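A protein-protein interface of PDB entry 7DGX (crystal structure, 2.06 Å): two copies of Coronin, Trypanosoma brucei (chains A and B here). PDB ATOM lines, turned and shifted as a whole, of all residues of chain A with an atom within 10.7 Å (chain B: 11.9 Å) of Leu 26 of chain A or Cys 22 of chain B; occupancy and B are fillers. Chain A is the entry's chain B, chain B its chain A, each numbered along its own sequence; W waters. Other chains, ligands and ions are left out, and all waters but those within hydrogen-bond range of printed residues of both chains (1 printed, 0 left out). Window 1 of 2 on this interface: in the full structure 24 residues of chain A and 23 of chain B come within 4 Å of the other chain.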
ATOM      1  N   GLU A  18      -6.305  24.949  40.418  1.00  0.00           N
ATOM      2  CA  GLU A  18      -6.262  25.540  39.084  1.00  0.00           C
ATOM      3  C   GLU A  18      -5.728  24.547  38.060  1.00  0.00           C
ATOM      4  O   GLU A  18      -6.157  24.551  36.900  1.00  0.00           O
ATOM      5  CB  GLU A  18      -5.408  26.808  39.098  1.00  0.00           C
ATOM      6  CG  GLU A  18      -6.201  28.100  38.981  1.00  0.00           C
ATOM      7  CD  GLU A  18      -6.725  28.345  37.579  1.00  0.00           C
ATOM      8  OE1 GLU A  18      -7.490  29.315  37.392  1.00  0.00           O
ATOM      9  OE2 GLU A  18      -6.373  27.574  36.662  1.00  0.00           O
ATOM     10  N   VAL A  19      -4.788  23.691  38.470  1.00  0.00           N
ATOM     11  CA  VAL A  19      -4.255  22.677  37.565  1.00  0.00           C
ATOM     12  C   VAL A  19      -5.345  21.685  37.178  1.00  0.00           C
ATOM     13  O   VAL A  19      -5.472  21.301  36.009  1.00  0.00           O
ATOM     14  CB  VAL A  19      -3.045  21.972  38.207  1.00  0.00           C
ATOM     15  CG1 VAL A  19      -2.742  20.660  37.496  1.00  0.00           C
ATOM     16  CG2 VAL A  19      -1.829  22.885  38.192  1.00  0.00           C
ATOM     17  N   GLN A  20      -6.156  21.266  38.152  1.00  0.00           N
ATOM     18  CA  GLN A  20      -7.214  20.301  37.870  1.00  0.00           C
ATOM     19  C   GLN A  20      -8.304  20.910  36.997  1.00  0.00           C
ATOM     20  O   GLN A  20      -8.860  20.230  36.126  1.00  0.00           O
ATOM     21  CB  GLN A  20      -7.802  19.771  39.177  1.00  0.00           C
ATOM     22  CG  GLN A  20      -8.572  18.469  39.022  1.00  0.00           C
ATOM     23  CD  GLN A  20      -7.896  17.501  38.069  1.00  0.00           C
ATOM     24  OE1 GLN A  20      -8.486  17.079  37.075  1.00  0.00           O
ATOM     25  NE2 GLN A  20      -6.654  17.140  38.372  1.00  0.00           N
ATOM     26  N   ARG A  21      -8.629  22.187  37.218  1.00  0.00           N
ATOM     27  CA  ARG A  21      -9.593  22.859  36.354  1.00  0.00           C
ATOM     28  C   ARG A  21      -9.080  22.944  34.923  1.00  0.00           C
ATOM     29  O   ARG A  21      -9.840  22.739  33.968  1.00  0.00           O
ATOM     30  CB  ARG A  21      -9.902  24.256  36.895  1.00  0.00           C
ATOM     31  CG  ARG A  21     -10.928  24.280  38.014  1.00  0.00           C
ATOM     32  CD  ARG A  21     -11.454  25.689  38.248  1.00  0.00           C
ATOM     33  NE  ARG A  21     -10.415  26.589  38.743  1.00  0.00           N
ATOM     34  CZ  ARG A  21     -10.074  26.703  40.022  1.00  0.00           C
ATOM     35  NH1 ARG A  21     -10.688  25.971  40.942  1.00  0.00           N
ATOM     36  NH2 ARG A  21      -9.119  27.548  40.383  1.00  0.00           N
ATOM     37  N   CYS A  22      -7.789  23.240  34.755  1.00  0.00           N
ATOM     38  CA  CYS A  22      -7.211  23.298  33.417  1.00  0.00           C
ATOM     39  C   CYS A  22      -7.129  21.912  32.789  1.00  0.00           C
ATOM     40  O   CYS A  22      -7.347  21.757  31.583  1.00  0.00           O
ATOM     41  CB  CYS A  22      -5.829  23.946  33.473  1.00  0.00           C
ATOM     42  SG  CYS A  22      -4.951  23.975  31.895  1.00  0.00           S
ATOM     43  N   ARG A  23      -6.819  20.892  33.594  1.00  0.00           N
ATOM     44  CA  ARG A  23      -6.710  19.538  33.062  1.00  0.00           C
ATOM     45  C   ARG A  23      -8.067  19.010  32.611  1.00  0.00           C
ATOM     46  O   ARG A  23      -8.173  18.378  31.553  1.00  0.00           O
ATOM     47  CB  ARG A  23      -6.092  18.610  34.108  1.00  0.00           C
ATOM     48  CG  ARG A  23      -6.193  17.133  33.765  1.00  0.00           C
ATOM     49  CD  ARG A  23      -5.338  16.286  34.692  1.00  0.00           C
ATOM     50  NE  ARG A  23      -3.922  16.630  34.597  1.00  0.00           N
ATOM     51  CZ  ARG A  23      -3.188  17.062  35.617  1.00  0.00           C
ATOM     52  NH1 ARG A  23      -3.734  17.202  36.817  1.00  0.00           N
ATOM     53  NH2 ARG A  23      -1.906  17.351  35.437  1.00  0.00           N
ATOM     54  N   GLU A  24      -9.117  19.260  33.399  1.00  0.00           N
ATOM     55  CA  GLU A  24     -10.450  18.807  33.016  1.00  0.00           C
ATOM     56  C   GLU A  24     -10.927  19.506  31.749  1.00  0.00           C
ATOM     57  O   GLU A  24     -11.573  18.885  30.896  1.00  0.00           O
ATOM     58  CB  GLU A  24     -11.432  19.041  34.164  1.00  0.00           C
ATOM     59  CG  GLU A  24     -11.333  18.018  35.283  1.00  0.00           C
ATOM     60  CD  GLU A  24     -12.245  18.339  36.451  1.00  0.00           C
ATOM     61  OE1 GLU A  24     -13.055  19.283  36.332  1.00  0.00           O
ATOM     62  OE2 GLU A  24     -12.151  17.649  37.488  1.00  0.00           O
ATOM     63  N   ASP A  25     -10.621  20.798  31.609  1.00  0.00           N
ATOM     64  CA  ASP A  25     -10.964  21.509  30.381  1.00  0.00           C
ATOM     65  C   ASP A  25     -10.170  20.971  29.198  1.00  0.00           C
ATOM     66  O   ASP A  25     -10.684  20.898  28.076  1.00  0.00           O
ATOM     67  CB  ASP A  25     -10.718  23.007  30.556  1.00  0.00           C
ATOM     68  CG  ASP A  25     -10.942  23.789  29.277  1.00  0.00           C
ATOM     69  OD1 ASP A  25     -12.114  23.962  28.881  1.00  0.00           O
ATOM     70  OD2 ASP A  25      -9.946  24.232  28.666  1.00  0.00           O
ATOM     71  N   LEU A  26      -8.915  20.582  29.435  1.00  0.00           N
ATOM     72  CA  LEU A  26      -8.092  20.039  28.359  1.00  0.00           C
ATOM     73  C   LEU A  26      -8.587  18.666  27.920  1.00  0.00           C
ATOM     74  O   LEU A  26      -8.627  18.369  26.720  1.00  0.00           O
ATOM     75  CB  LEU A  26      -6.632  19.967  28.808  1.00  0.00           C
ATOM     76  CG  LEU A  26      -5.685  19.144  27.933  1.00  0.00           C
ATOM     77  CD1 LEU A  26      -5.559  19.760  26.548  1.00  0.00           C
ATOM     78  CD2 LEU A  26      -4.321  19.013  28.595  1.00  0.00           C
ATOM     79  N   GLN A  27      -8.967  17.815  28.877  1.00  0.00           N
ATOM     80  CA  GLN A  27      -9.442  16.479  28.531  1.00  0.00           C
ATOM     81  C   GLN A  27     -10.746  16.531  27.744  1.00  0.00           C
ATOM     82  O   GLN A  27     -10.986  15.669  26.891  1.00  0.00           O
ATOM     83  CB  GLN A  27      -9.615  15.638  29.795  1.00  0.00           C
ATOM     84  CG  GLN A  27      -8.305  15.272  30.471  1.00  0.00           C
ATOM     85  CD  GLN A  27      -8.509  14.476  31.744  1.00  0.00           C
ATOM     86  OE1 GLN A  27      -9.628  14.358  32.243  1.00  0.00           O
ATOM     87  NE2 GLN A  27      -7.425  13.926  32.276  1.00  0.00           N
ATOM     88  N   LYS A  28     -11.596  17.524  28.015  1.00  0.00           N
ATOM     89  CA  LYS A  28     -12.814  17.682  27.226  1.00  0.00           C
ATOM     90  C   LYS A  28     -12.489  18.070  25.789  1.00  0.00           C
ATOM     91  O   LYS A  28     -13.090  17.543  24.845  1.00  0.00           O
ATOM     92  CB  LYS A  28     -13.727  18.724  27.872  1.00  0.00           C
ATOM     93  N   LYS A  29     -11.535  18.987  25.603  1.00  0.00           N
ATOM     94  CA  LYS A  29     -11.137  19.375  24.255  1.00  0.00           C
ATOM     95  C   LYS A  29     -10.391  18.253  23.545  1.00  0.00           C
ATOM     96  O   LYS A  29     -10.445  18.157  22.313  1.00  0.00           O
ATOM     97  CB  LYS A  29     -10.284  20.642  24.307  1.00  0.00           C
ATOM     98  CG  LYS A  29     -11.092  21.908  24.545  1.00  0.00           C
ATOM     99  CD  LYS A  29     -10.261  22.991  25.212  1.00  0.00           C
ATOM    100  CE  LYS A  29     -11.083  24.251  25.435  1.00  0.00           C
ATOM    101  NZ  LYS A  29     -10.385  25.229  26.314  1.00  0.00           N
ATOM    102  N   GLU A  30      -9.689  17.401  24.297  1.00  0.00           N
ATOM    103  CA  GLU A  30      -9.060  16.233  23.690  1.00  0.00           C
ATOM    104  C   GLU A  30     -10.107  15.247  23.189  1.00  0.00           C
ATOM    105  O   GLU A  30      -9.950  14.659  22.112  1.00  0.00           O
ATOM    106  CB  GLU A  30      -8.124  15.556  24.691  1.00  0.00           C
ATOM    107  CG  GLU A  30      -6.806  16.280  24.905  1.00  0.00           C
ATOM    108  CD  GLU A  30      -5.945  15.613  25.960  1.00  0.00           C
ATOM    109  OE1 GLU A  30      -6.478  14.783  26.726  1.00  0.00           O
ATOM    110  OE2 GLU A  30      -4.736  15.920  26.023  1.00  0.00           O
ATOM    111  N   SER A  31     -11.182  15.053  23.959  1.00  0.00           N
ATOM    112  CA  SER A  31     -12.257  14.171  23.520  1.00  0.00           C
ATOM    113  C   SER A  31     -12.937  14.703  22.266  1.00  0.00           C
ATOM    114  O   SER A  31     -13.382  13.917  21.421  1.00  0.00           O
ATOM    115  CB  SER A  31     -13.280  13.989  24.642  1.00  0.00           C
ATOM    116  OG  SER A  31     -12.714  13.300  25.743  1.00  0.00           O
ATOM    117  N   LEU A  32     -13.028  16.027  22.127  1.00  0.00           N
ATOM    118  CA  LEU A  32     -13.599  16.606  20.915  1.00  0.00           C
ATOM    119  C   LEU A  32     -12.727  16.307  19.703  1.00  0.00           C
ATOM    120  O   LEU A  32     -13.240  16.047  18.607  1.00  0.00           O
ATOM    121  CB  LEU A  32     -13.780  18.115  21.088  1.00  0.00           C
ATOM    122  CG  LEU A  32     -15.187  18.612  21.425  1.00  0.00           C
ATOM    123  CD1 LEU A  32     -15.756  17.868  22.623  1.00  0.00           C
ATOM    124  CD2 LEU A  32     -15.178  20.113  21.679  1.00  0.00           C
ATOM    125  N   VAL A  33     -11.404  16.342  19.880  1.00  0.00           N
ATOM    126  CA  VAL A  33     -10.493  15.998  18.793  1.00  0.00           C
ATOM    127  C   VAL A  33     -10.666  14.536  18.398  1.00  0.00           C
ATOM    128  O   VAL A  33     -10.666  14.194  17.208  1.00  0.00           O
ATOM    129  CB  VAL A  33      -9.040  16.311  19.201  1.00  0.00           C
ATOM    130  CG1 VAL A  33      -8.054  15.579  18.299  1.00  0.00           C
ATOM    131  CG2 VAL A  33      -8.790  17.811  19.168  1.00  0.00           C
ATOM    132  N   MET A  34     -10.829  13.655  19.388  1.00  0.00           N
ATOM    133  CA  MET A  34     -10.991  12.233  19.100  1.00  0.00           C
ATOM    134  C   MET A  34     -12.268  11.966  18.314  1.00  0.00           C
ATOM    135  O   MET A  34     -12.273  11.153  17.381  1.00  0.00           O
ATOM    136  CB  MET A  34     -10.986  11.431  20.401  1.00  0.00           C
ATOM    137  CG  MET A  34      -9.654  11.431  21.131  1.00  0.00           C
ATOM    138  SD  MET A  34      -9.618  10.234  22.477  1.00  0.00           S
ATOM    139  CE  MET A  34      -9.953  11.289  23.884  1.00  0.00           C
ATOM    140  N   GLY B  13      -8.134  21.067  12.733  1.00  0.00           N
ATOM    141  CA  GLY B  13      -6.995  21.951  12.921  1.00  0.00           C
ATOM    142  C   GLY B  13      -7.241  23.000  13.987  1.00  0.00           C
ATOM    143  O   GLY B  13      -6.348  23.318  14.776  1.00  0.00           O
ATOM    144  N   GLN B  14      -8.456  23.548  14.028  1.00  0.00           N
ATOM    145  CA  GLN B  14      -8.795  24.511  15.071  1.00  0.00           C
ATOM    146  C   GLN B  14      -8.856  23.841  16.438  1.00  0.00           C
ATOM    147  O   GLN B  14      -8.371  24.396  17.430  1.00  0.00           O
ATOM    148  CB  GLN B  14     -10.126  25.191  14.746  1.00  0.00           C
ATOM    149  CG  GLN B  14     -10.628  26.124  15.839  1.00  0.00           C
ATOM    150  CD  GLN B  14     -12.117  25.978  16.096  1.00  0.00           C
ATOM    151  OE1 GLN B  14     -12.941  26.529  15.366  1.00  0.00           O
ATOM    152  NE2 GLN B  14     -12.467  25.234  17.138  1.00  0.00           N
ATOM    153  N   GLN B  15      -9.412  22.642  16.492  1.00  0.00           N
ATOM    154  CA  GLN B  15      -9.551  21.918  17.767  1.00  0.00           C
ATOM    155  C   GLN B  15      -8.170  21.535  18.283  1.00  0.00           C
ATOM    156  O   GLN B  15      -7.919  21.694  19.441  1.00  0.00           O
ATOM    157  CB  GLN B  15     -10.468  20.716  17.588  1.00  0.00           C
ATOM    158  CG  GLN B  15     -11.919  21.068  17.375  1.00  0.00           C
ATOM    159  CD  GLN B  15     -12.825  19.890  17.128  1.00  0.00           C
ATOM    160  OE1 GLN B  15     -13.979  19.888  17.501  1.00  0.00           O
ATOM    161  NE2 GLN B  15     -12.324  18.885  16.459  1.00  0.00           N
ATOM    162  N   GLN B  16      -7.314  21.039  17.419  1.00  0.00           N
ATOM    163  CA  GLN B  16      -5.978  20.642  17.846  1.00  0.00           C
ATOM    164  C   GLN B  16      -5.166  21.844  18.312  1.00  0.00           C
ATOM    165  O   GLN B  16      -4.418  21.751  19.291  1.00  0.00           O
ATOM    166  CB  GLN B  16      -5.256  19.913  16.712  1.00  0.00           C
ATOM    167  CG  GLN B  16      -5.186  18.405  16.888  1.00  0.00           C
ATOM    168  CD  GLN B  16      -4.382  17.997  18.106  1.00  0.00           C
ATOM    169  OE1 GLN B  16      -4.917  17.407  19.046  1.00  0.00           O
ATOM    170  NE2 GLN B  16      -3.091  18.306  18.097  1.00  0.00           N
ATOM    171  N   ALA B  17      -5.304  22.981  17.625  1.00  0.00           N
ATOM    172  CA  ALA B  17      -4.584  24.183  18.034  1.00  0.00           C
ATOM    173  C   ALA B  17      -5.023  24.643  19.419  1.00  0.00           C
ATOM    174  O   ALA B  17      -4.213  25.162  20.196  1.00  0.00           O
ATOM    175  CB  ALA B  17      -4.791  25.295  17.008  1.00  0.00           C
ATOM    176  N   GLU B  18      -6.304  24.459  19.745  1.00  0.00           N
ATOM    177  CA  GLU B  18      -6.783  24.803  21.080  1.00  0.00           C
ATOM    178  C   GLU B  18      -6.257  23.824  22.123  1.00  0.00           C
ATOM    179  O   GLU B  18      -5.982  24.213  23.264  1.00  0.00           O
ATOM    180  CB  GLU B  18      -8.312  24.840  21.091  1.00  0.00           C
ATOM    181  CG  GLU B  18      -8.929  25.063  22.461  1.00  0.00           C
ATOM    182  CD  GLU B  18      -8.634  26.441  23.022  1.00  0.00           C
ATOM    183  OE1 GLU B  18      -8.694  26.604  24.259  1.00  0.00           O
ATOM    184  OE2 GLU B  18      -8.345  27.361  22.229  1.00  0.00           O
ATOM    185  N   VAL B  19      -6.107  22.552  21.747  1.00  0.00           N
ATOM    186  CA  VAL B  19      -5.578  21.556  22.677  1.00  0.00           C
ATOM    187  C   VAL B  19      -4.138  21.889  23.046  1.00  0.00           C
ATOM    188  O   VAL B  19      -3.757  21.863  24.222  1.00  0.00           O
ATOM    189  CB  VAL B  19      -5.699  20.144  22.075  1.00  0.00           C
ATOM    190  CG1 VAL B  19      -4.689  19.199  22.711  1.00  0.00           C
ATOM    191  CG2 VAL B  19      -7.114  19.614  22.248  1.00  0.00           C
ATOM    192  N   GLN B  20      -3.316  22.214  22.044  1.00  0.00           N
ATOM    193  CA  GLN B  20      -1.927  22.571  22.316  1.00  0.00           C
ATOM    194  C   GLN B  20      -1.828  23.852  23.133  1.00  0.00           C
ATOM    195  O   GLN B  20      -0.925  23.986  23.967  1.00  0.00           O
ATOM    196  CB  GLN B  20      -1.152  22.714  21.005  1.00  0.00           C
ATOM    197  CG  GLN B  20      -1.370  21.575  20.022  1.00  0.00           C
ATOM    198  CD  GLN B  20      -0.418  20.415  20.240  1.00  0.00           C
ATOM    199  OE1 GLN B  20       0.024  20.159  21.361  1.00  0.00           O
ATOM    200  NE2 GLN B  20      -0.098  19.703  19.166  1.00  0.00           N
ATOM    201  N   ARG B  21      -2.742  24.800  22.911  1.00  0.00           N
ATOM    202  CA  ARG B  21      -2.757  26.012  23.725  1.00  0.00           C
ATOM    203  C   ARG B  21      -3.095  25.692  25.176  1.00  0.00           C
ATOM    204  O   ARG B  21      -2.494  26.251  26.101  1.00  0.00           O
ATOM    205  CB  ARG B  21      -3.754  27.019  23.153  1.00  0.00           C
ATOM    206  CG  ARG B  21      -3.194  27.894  22.044  1.00  0.00           C
ATOM    207  CD  ARG B  21      -4.129  29.054  21.735  1.00  0.00           C
ATOM    208  NE  ARG B  21      -5.424  28.594  21.237  1.00  0.00           N
ATOM    209  CZ  ARG B  21      -5.716  28.435  19.951  1.00  0.00           C
ATOM    210  NH1 ARG B  21      -4.805  28.699  19.024  1.00  0.00           N
ATOM    211  NH2 ARG B  21      -6.920  28.012  19.589  1.00  0.00           N
ATOM    212  N   CYS B  22      -4.057  24.792  25.395  1.00  0.00           N
ATOM    213  CA  CYS B  22      -4.406  24.398  26.755  1.00  0.00           C
ATOM    214  C   CYS B  22      -3.290  23.598  27.412  1.00  0.00           C
ATOM    215  O   CYS B  22      -3.106  23.681  28.631  1.00  0.00           O
ATOM    216  CB  CYS B  22      -5.706  23.594  26.753  1.00  0.00           C
ATOM    217  SG  CYS B  22      -7.180  24.566  26.368  1.00  0.00           S
ATOM    218  N   ARG B  23      -2.541  22.819  26.627  1.00  0.00           N
ATOM    219  CA  ARG B  23      -1.410  22.087  27.186  1.00  0.00           C
ATOM    220  C   ARG B  23      -0.318  23.040  27.656  1.00  0.00           C
ATOM    221  O   ARG B  23       0.329  22.795  28.680  1.00  0.00           O
ATOM    222  CB  ARG B  23      -0.861  21.097  26.159  1.00  0.00           C
ATOM    223  CG  ARG B  23      -1.681  19.822  26.037  1.00  0.00           C
ATOM    224  CD  ARG B  23      -1.172  18.931  24.914  1.00  0.00           C
ATOM    225  NE  ARG B  23      -2.033  17.767  24.721  1.00  0.00           N
ATOM    226  CZ  ARG B  23      -2.034  17.013  23.626  1.00  0.00           C
ATOM    227  NH1 ARG B  23      -1.219  17.298  22.621  1.00  0.00           N
ATOM    228  NH2 ARG B  23      -2.854  15.974  23.537  1.00  0.00           N
ATOM    229  N   GLU B  24      -0.101  24.133  26.920  1.00  0.00           N
ATOM    230  CA  GLU B  24       0.850  25.145  27.368  1.00  0.00           C
ATOM    231  C   GLU B  24       0.385  25.793  28.666  1.00  0.00           C
ATOM    232  O   GLU B  24       1.198  26.085  29.549  1.00  0.00           O
ATOM    233  CB  GLU B  24       1.045  26.202  26.281  1.00  0.00           C
ATOM    234  CG  GLU B  24       1.677  25.677  25.003  1.00  0.00           C
ATOM    235  CD  GLU B  24       1.647  26.694  23.879  1.00  0.00           C
ATOM    236  OE1 GLU B  24       1.196  27.835  24.119  1.00  0.00           O
ATOM    237  OE2 GLU B  24       2.072  26.354  22.755  1.00  0.00           O
ATOM    238  N   ASP B  25      -0.924  26.025  28.796  1.00  0.00           N
ATOM    239  CA  ASP B  25      -1.455  26.591  30.032  1.00  0.00           C
ATOM    240  C   ASP B  25      -1.275  25.627  31.198  1.00  0.00           C
ATOM    241  O   ASP B  25      -0.971  26.047  32.320  1.00  0.00           O
ATOM    242  CB  ASP B  25      -2.931  26.946  29.857  1.00  0.00           C
ATOM    243  CG  ASP B  25      -3.143  28.129  28.932  1.00  0.00           C
ATOM    244  OD1 ASP B  25      -2.237  28.983  28.839  1.00  0.00           O
ATOM    245  OD2 ASP B  25      -4.216  28.203  28.298  1.00  0.00           O
ATOM    246  N   LEU B  26      -1.457  24.328  30.949  1.00  0.00           N
ATOM    247  CA  LEU B  26      -1.318  23.343  32.018  1.00  0.00           C
ATOM    248  C   LEU B  26       0.123  23.253  32.505  1.00  0.00           C
ATOM    249  O   LEU B  26       0.368  23.094  33.706  1.00  0.00           O
ATOM    250  CB  LEU B  26      -1.809  21.978  31.538  1.00  0.00           C
ATOM    251  CG  LEU B  26      -1.789  20.855  32.576  1.00  0.00           C
ATOM    252  CD1 LEU B  26      -2.688  21.201  33.753  1.00  0.00           C
ATOM    253  CD2 LEU B  26      -2.198  19.531  31.951  1.00  0.00           C
ATOM    254  N   GLN B  27       1.057  23.378  31.582  1.00  0.00           N
ATOM    255  CA  GLN B  27       2.476  23.286  31.956  1.00  0.00           C
ATOM    256  C   GLN B  27       2.834  24.476  32.844  1.00  0.00           C
ATOM    257  O   GLN B  27       3.490  24.273  33.804  1.00  0.00           O
ATOM    258  CB  GLN B  27       3.343  23.160  30.709  1.00  0.00           C
ATOM    259  CG  GLN B  27       3.302  21.786  30.041  1.00  0.00           C
ATOM    260  CD  GLN B  27       4.273  20.768  30.595  1.00  0.00           C
ATOM    261  OE1 GLN B  27       4.778  20.907  31.696  1.00  0.00           O
ATOM    262  NE2 GLN B  27       4.537  19.717  29.846  1.00  0.00           N
ATOM    263  N   LYS B  28       2.365  25.662  32.520  1.00  0.00           N
ATOM    264  CA  LYS B  28       2.675  26.845  33.314  1.00  0.00           C
ATOM    265  C   LYS B  28       2.062  26.752  34.706  1.00  0.00           C
ATOM    266  O   LYS B  28       2.685  27.159  35.694  1.00  0.00           O
ATOM    267  CB  LYS B  28       2.187  28.101  32.594  1.00  0.00           C
ATOM    268  N   LYS B  29       0.843  26.219  34.806  1.00  0.00           N
ATOM    269  CA  LYS B  29       0.200  26.088  36.108  1.00  0.00           C
ATOM    270  C   LYS B  29       0.831  24.978  36.938  1.00  0.00           C
ATOM    271  O   LYS B  29       0.904  25.090  38.167  1.00  0.00           O
ATOM    272  CB  LYS B  29      -1.297  25.842  35.932  1.00  0.00           C
ATOM    273  CG  LYS B  29      -2.028  26.990  35.255  1.00  0.00           C
ATOM    274  CD  LYS B  29      -3.465  26.627  34.931  1.00  0.00           C
ATOM    275  CE  LYS B  29      -4.193  27.800  34.292  1.00  0.00           C
ATOM    276  NZ  LYS B  29      -4.243  28.977  35.202  1.00  0.00           N
ATOM    277  N   GLU B  30       1.289  23.904  36.291  1.00  0.00           N
ATOM    278  CA  GLU B  30       1.988  22.849  37.018  1.00  0.00           C
ATOM    279  C   GLU B  30       3.337  23.337  37.532  1.00  0.00           C
ATOM    280  O   GLU B  30       3.767  22.950  38.625  1.00  0.00           O
ATOM    281  CB  GLU B  30       2.170  21.623  36.122  1.00  0.00           C
ATOM    282  CG  GLU B  30       0.952  20.719  36.039  1.00  0.00           C
ATOM    283  CD  GLU B  30       1.246  19.416  35.321  1.00  0.00           C
ATOM    284  OE1 GLU B  30       2.319  19.316  34.689  1.00  0.00           O
ATOM    285  OE2 GLU B  30       0.405  18.496  35.385  1.00  0.00           O
ATOM    286  N   SER B  31       4.017  24.184  36.755  1.00  0.00           N
ATOM    287  CA  SER B  31       5.295  24.732  37.198  1.00  0.00           C
ATOM    288  C   SER B  31       5.123  25.590  38.445  1.00  0.00           C
ATOM    289  O   SER B  31       5.991  25.601  39.326  1.00  0.00           O
ATOM    290  CB  SER B  31       5.937  25.543  36.072  1.00  0.00           C
ATOM    291  OG  SER B  31       7.195  26.059  36.468  1.00  0.00           O
HETATM  292  O   HOH W   1      -7.365  23.821  29.640  1.00  0.00           O
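The side-chain sulfur (SG) of Cys 22 of chain A sits at hydrogen-bond distance from the backbone NH (N) of Leu 26 of chain B (3.6 Å).
The side-chain sulfur of Cys 22 of chain B lies within hydrogen-bond range of the side-chain carboxylate of Asp 25 of chain A (3.6 Å).
The backbone carbonyl oxygen of Cys 22 of chain B sits at hydrogen-bond distance from the side-chain sulfur of Cys 22 of chain A (3.8 Å).
NZ of Lys 29 of chain A lies within salt-bridge range of OE1 of Glu 18 of chain B (3.0 Å).
The side-chain sulfur (SG) of Cys 22 of chain B is in hydrogen-bond range of the side-chain amino group (NZ) of Lys 29 of chain A (3.3 Å).
NH2 of Arg 23 of chain B lies within salt-bridge range of OE2 of Glu 30 of chain A.
OE2 of Glu 30 of chain B lies within salt-bridge range of NH2 of Arg 23 of chain A, 2.6 Å away.
OE2 of Glu 18 of chain A lies within salt-bridge range of NZ of Lys 29 of chain B (2.9 Å).
The side-chain amide nitrogen (NE2) of Gln 16 of chain B sits close to the side-chain amide nitrogen (NE2) of Gln 20 of chain B, 3.5 Å away.
OD2 of Asp 25 of chain A lies within salt-bridge range of NZ of Lys 29 of chain A, at 2.6 Å.
OE1 of Gln 20 of chain B sits at hydrogen-bond distance from NH1 of Arg 23 of chain B.
NH1 of Arg 23 of chain A sits close to NE2 of Gln 20 of chain A (3.3 Å).
The side-chain carboxylate (OE1) of Glu 18 of chain A is in salt-bridge range of the guanidinium group (NH2) of Arg 21 of chain A, at 3.8 Å.
O of Val 19 of chain A touches CD1 of Leu 26 of chain B, 3.6 Å away.
O of Lys 29 of chain B touches CG2 of Val 19 of chain A, 3.5 Å away.
N of Glu 30 of chain B touches CG2 of Val 19 of chain A, at 3.8 Å.
Val 19 of chain B touches Leu 26 of chain A (O to CD1, 3.6 Å).
Leu 26 of chain A touches Cys 22 of chain B.
Lys 29 of chain A touches Val 19 of chain B (O to CG2, 3.6 Å).
CB of Gln 15 of chain B touches CG2 of Val 33 of chain A, 3.7 Å away.
Val 33 of chain A touches Gln 16 of chain B.
Val 33 of chain A touches Val 19 of chain B (CG2 to CG2, 3.9 Å).
Of the printed residues of chain B, Glu 18 of chain A touches Lys 29 (2.9 Å).
Cys 22 of chain A touches three residues of chain B.
Of the printed residues of chain B, Arg 23 of chain A touches Glu 30 (2.6 Å).
Of the printed residues of chain B, Leu 26 of chain A touches Val 19 (3.6 Å), Cys 22 (3.8 Å) and Arg 23 (3.8 Å).
No residue of chain B comes within 4 Å of Gln 27 of chain A.
Lys 28 of chain A touches none of the printed residues of chain B.
Lys 29 of chain A touches just these residues of chain B: Glu 18 (3.0 Å), Val 19 (3.6 Å) and Cys 22 (3.3 Å).
Of chain B, only Val 19 (3.97 Å) and Arg 23 (3.1 Å) come within 4 Å of Glu 30 of chain A.
Printed residues of chain A within 4 Å of Gln 15 of chain B: Leu 32 and Val 33.
Printed residues of chain A within 4 Å of Gln 16 of chain B: Val 33 (3.7 Å).
Cys 22 of chain B touches just these residues of chain A: Cys 22, Asp 25, Leu 26 and Lys 29.
Of chain A, only Leu 26 and Glu 30 come within 4 Å of Arg 23 of chain B.
No residue of chain A comes within 4 Å of Asp 25 of chain B.
Lys 28 of chain B touches none of the printed residues of chain A.
The nearest printed residue of chain B that does not touch Leu 26 of chain A is Leu 26 of chain B (4.005 Å).
Hydrophobic or aromatic side chains of chain A within 4 Å of the printed part of chain B: Val 19, Leu 26 and Val 33.
Printed residues of chain B that touch a printed residue of chain A: Gln 15, Gln 16, Glu 18, Val 19, Cys 22, Arg 23, Leu 26, Lys 29 and Glu 30.
Along chain B the printed residues that touch a printed residue of chain A span positions 15 to 30.
Among the printed residues, 21 pairs touch across the chains.
Glu 18 of chain A touches Lys 29 of chain B, and with the chains exchanged Lys 29 of chain A touches Glu 18 of chain B.
Val 19 of chain A touches Leu 26 of chain B, and with the chains exchanged Leu 26 of chain A touches Val 19 of chain B.
Cys 22 of chain A touches its own counterpart, Cys 22 of chain B.
Of the 21 pairs that touch across the chains among the printed residues, 15 have their exchanged pair printed and touching as well.
Water W1 lies within hydrogen-bond range of the side-chain carboxylate (OD2) of Asp 25 of chain A (2.8 Å), the backbone carbonyl oxygen (O) of Cys 22 of chain A (2.8 Å) and the side-chain sulfur (SG) of Cys 22 of chain B (3.4 Å).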
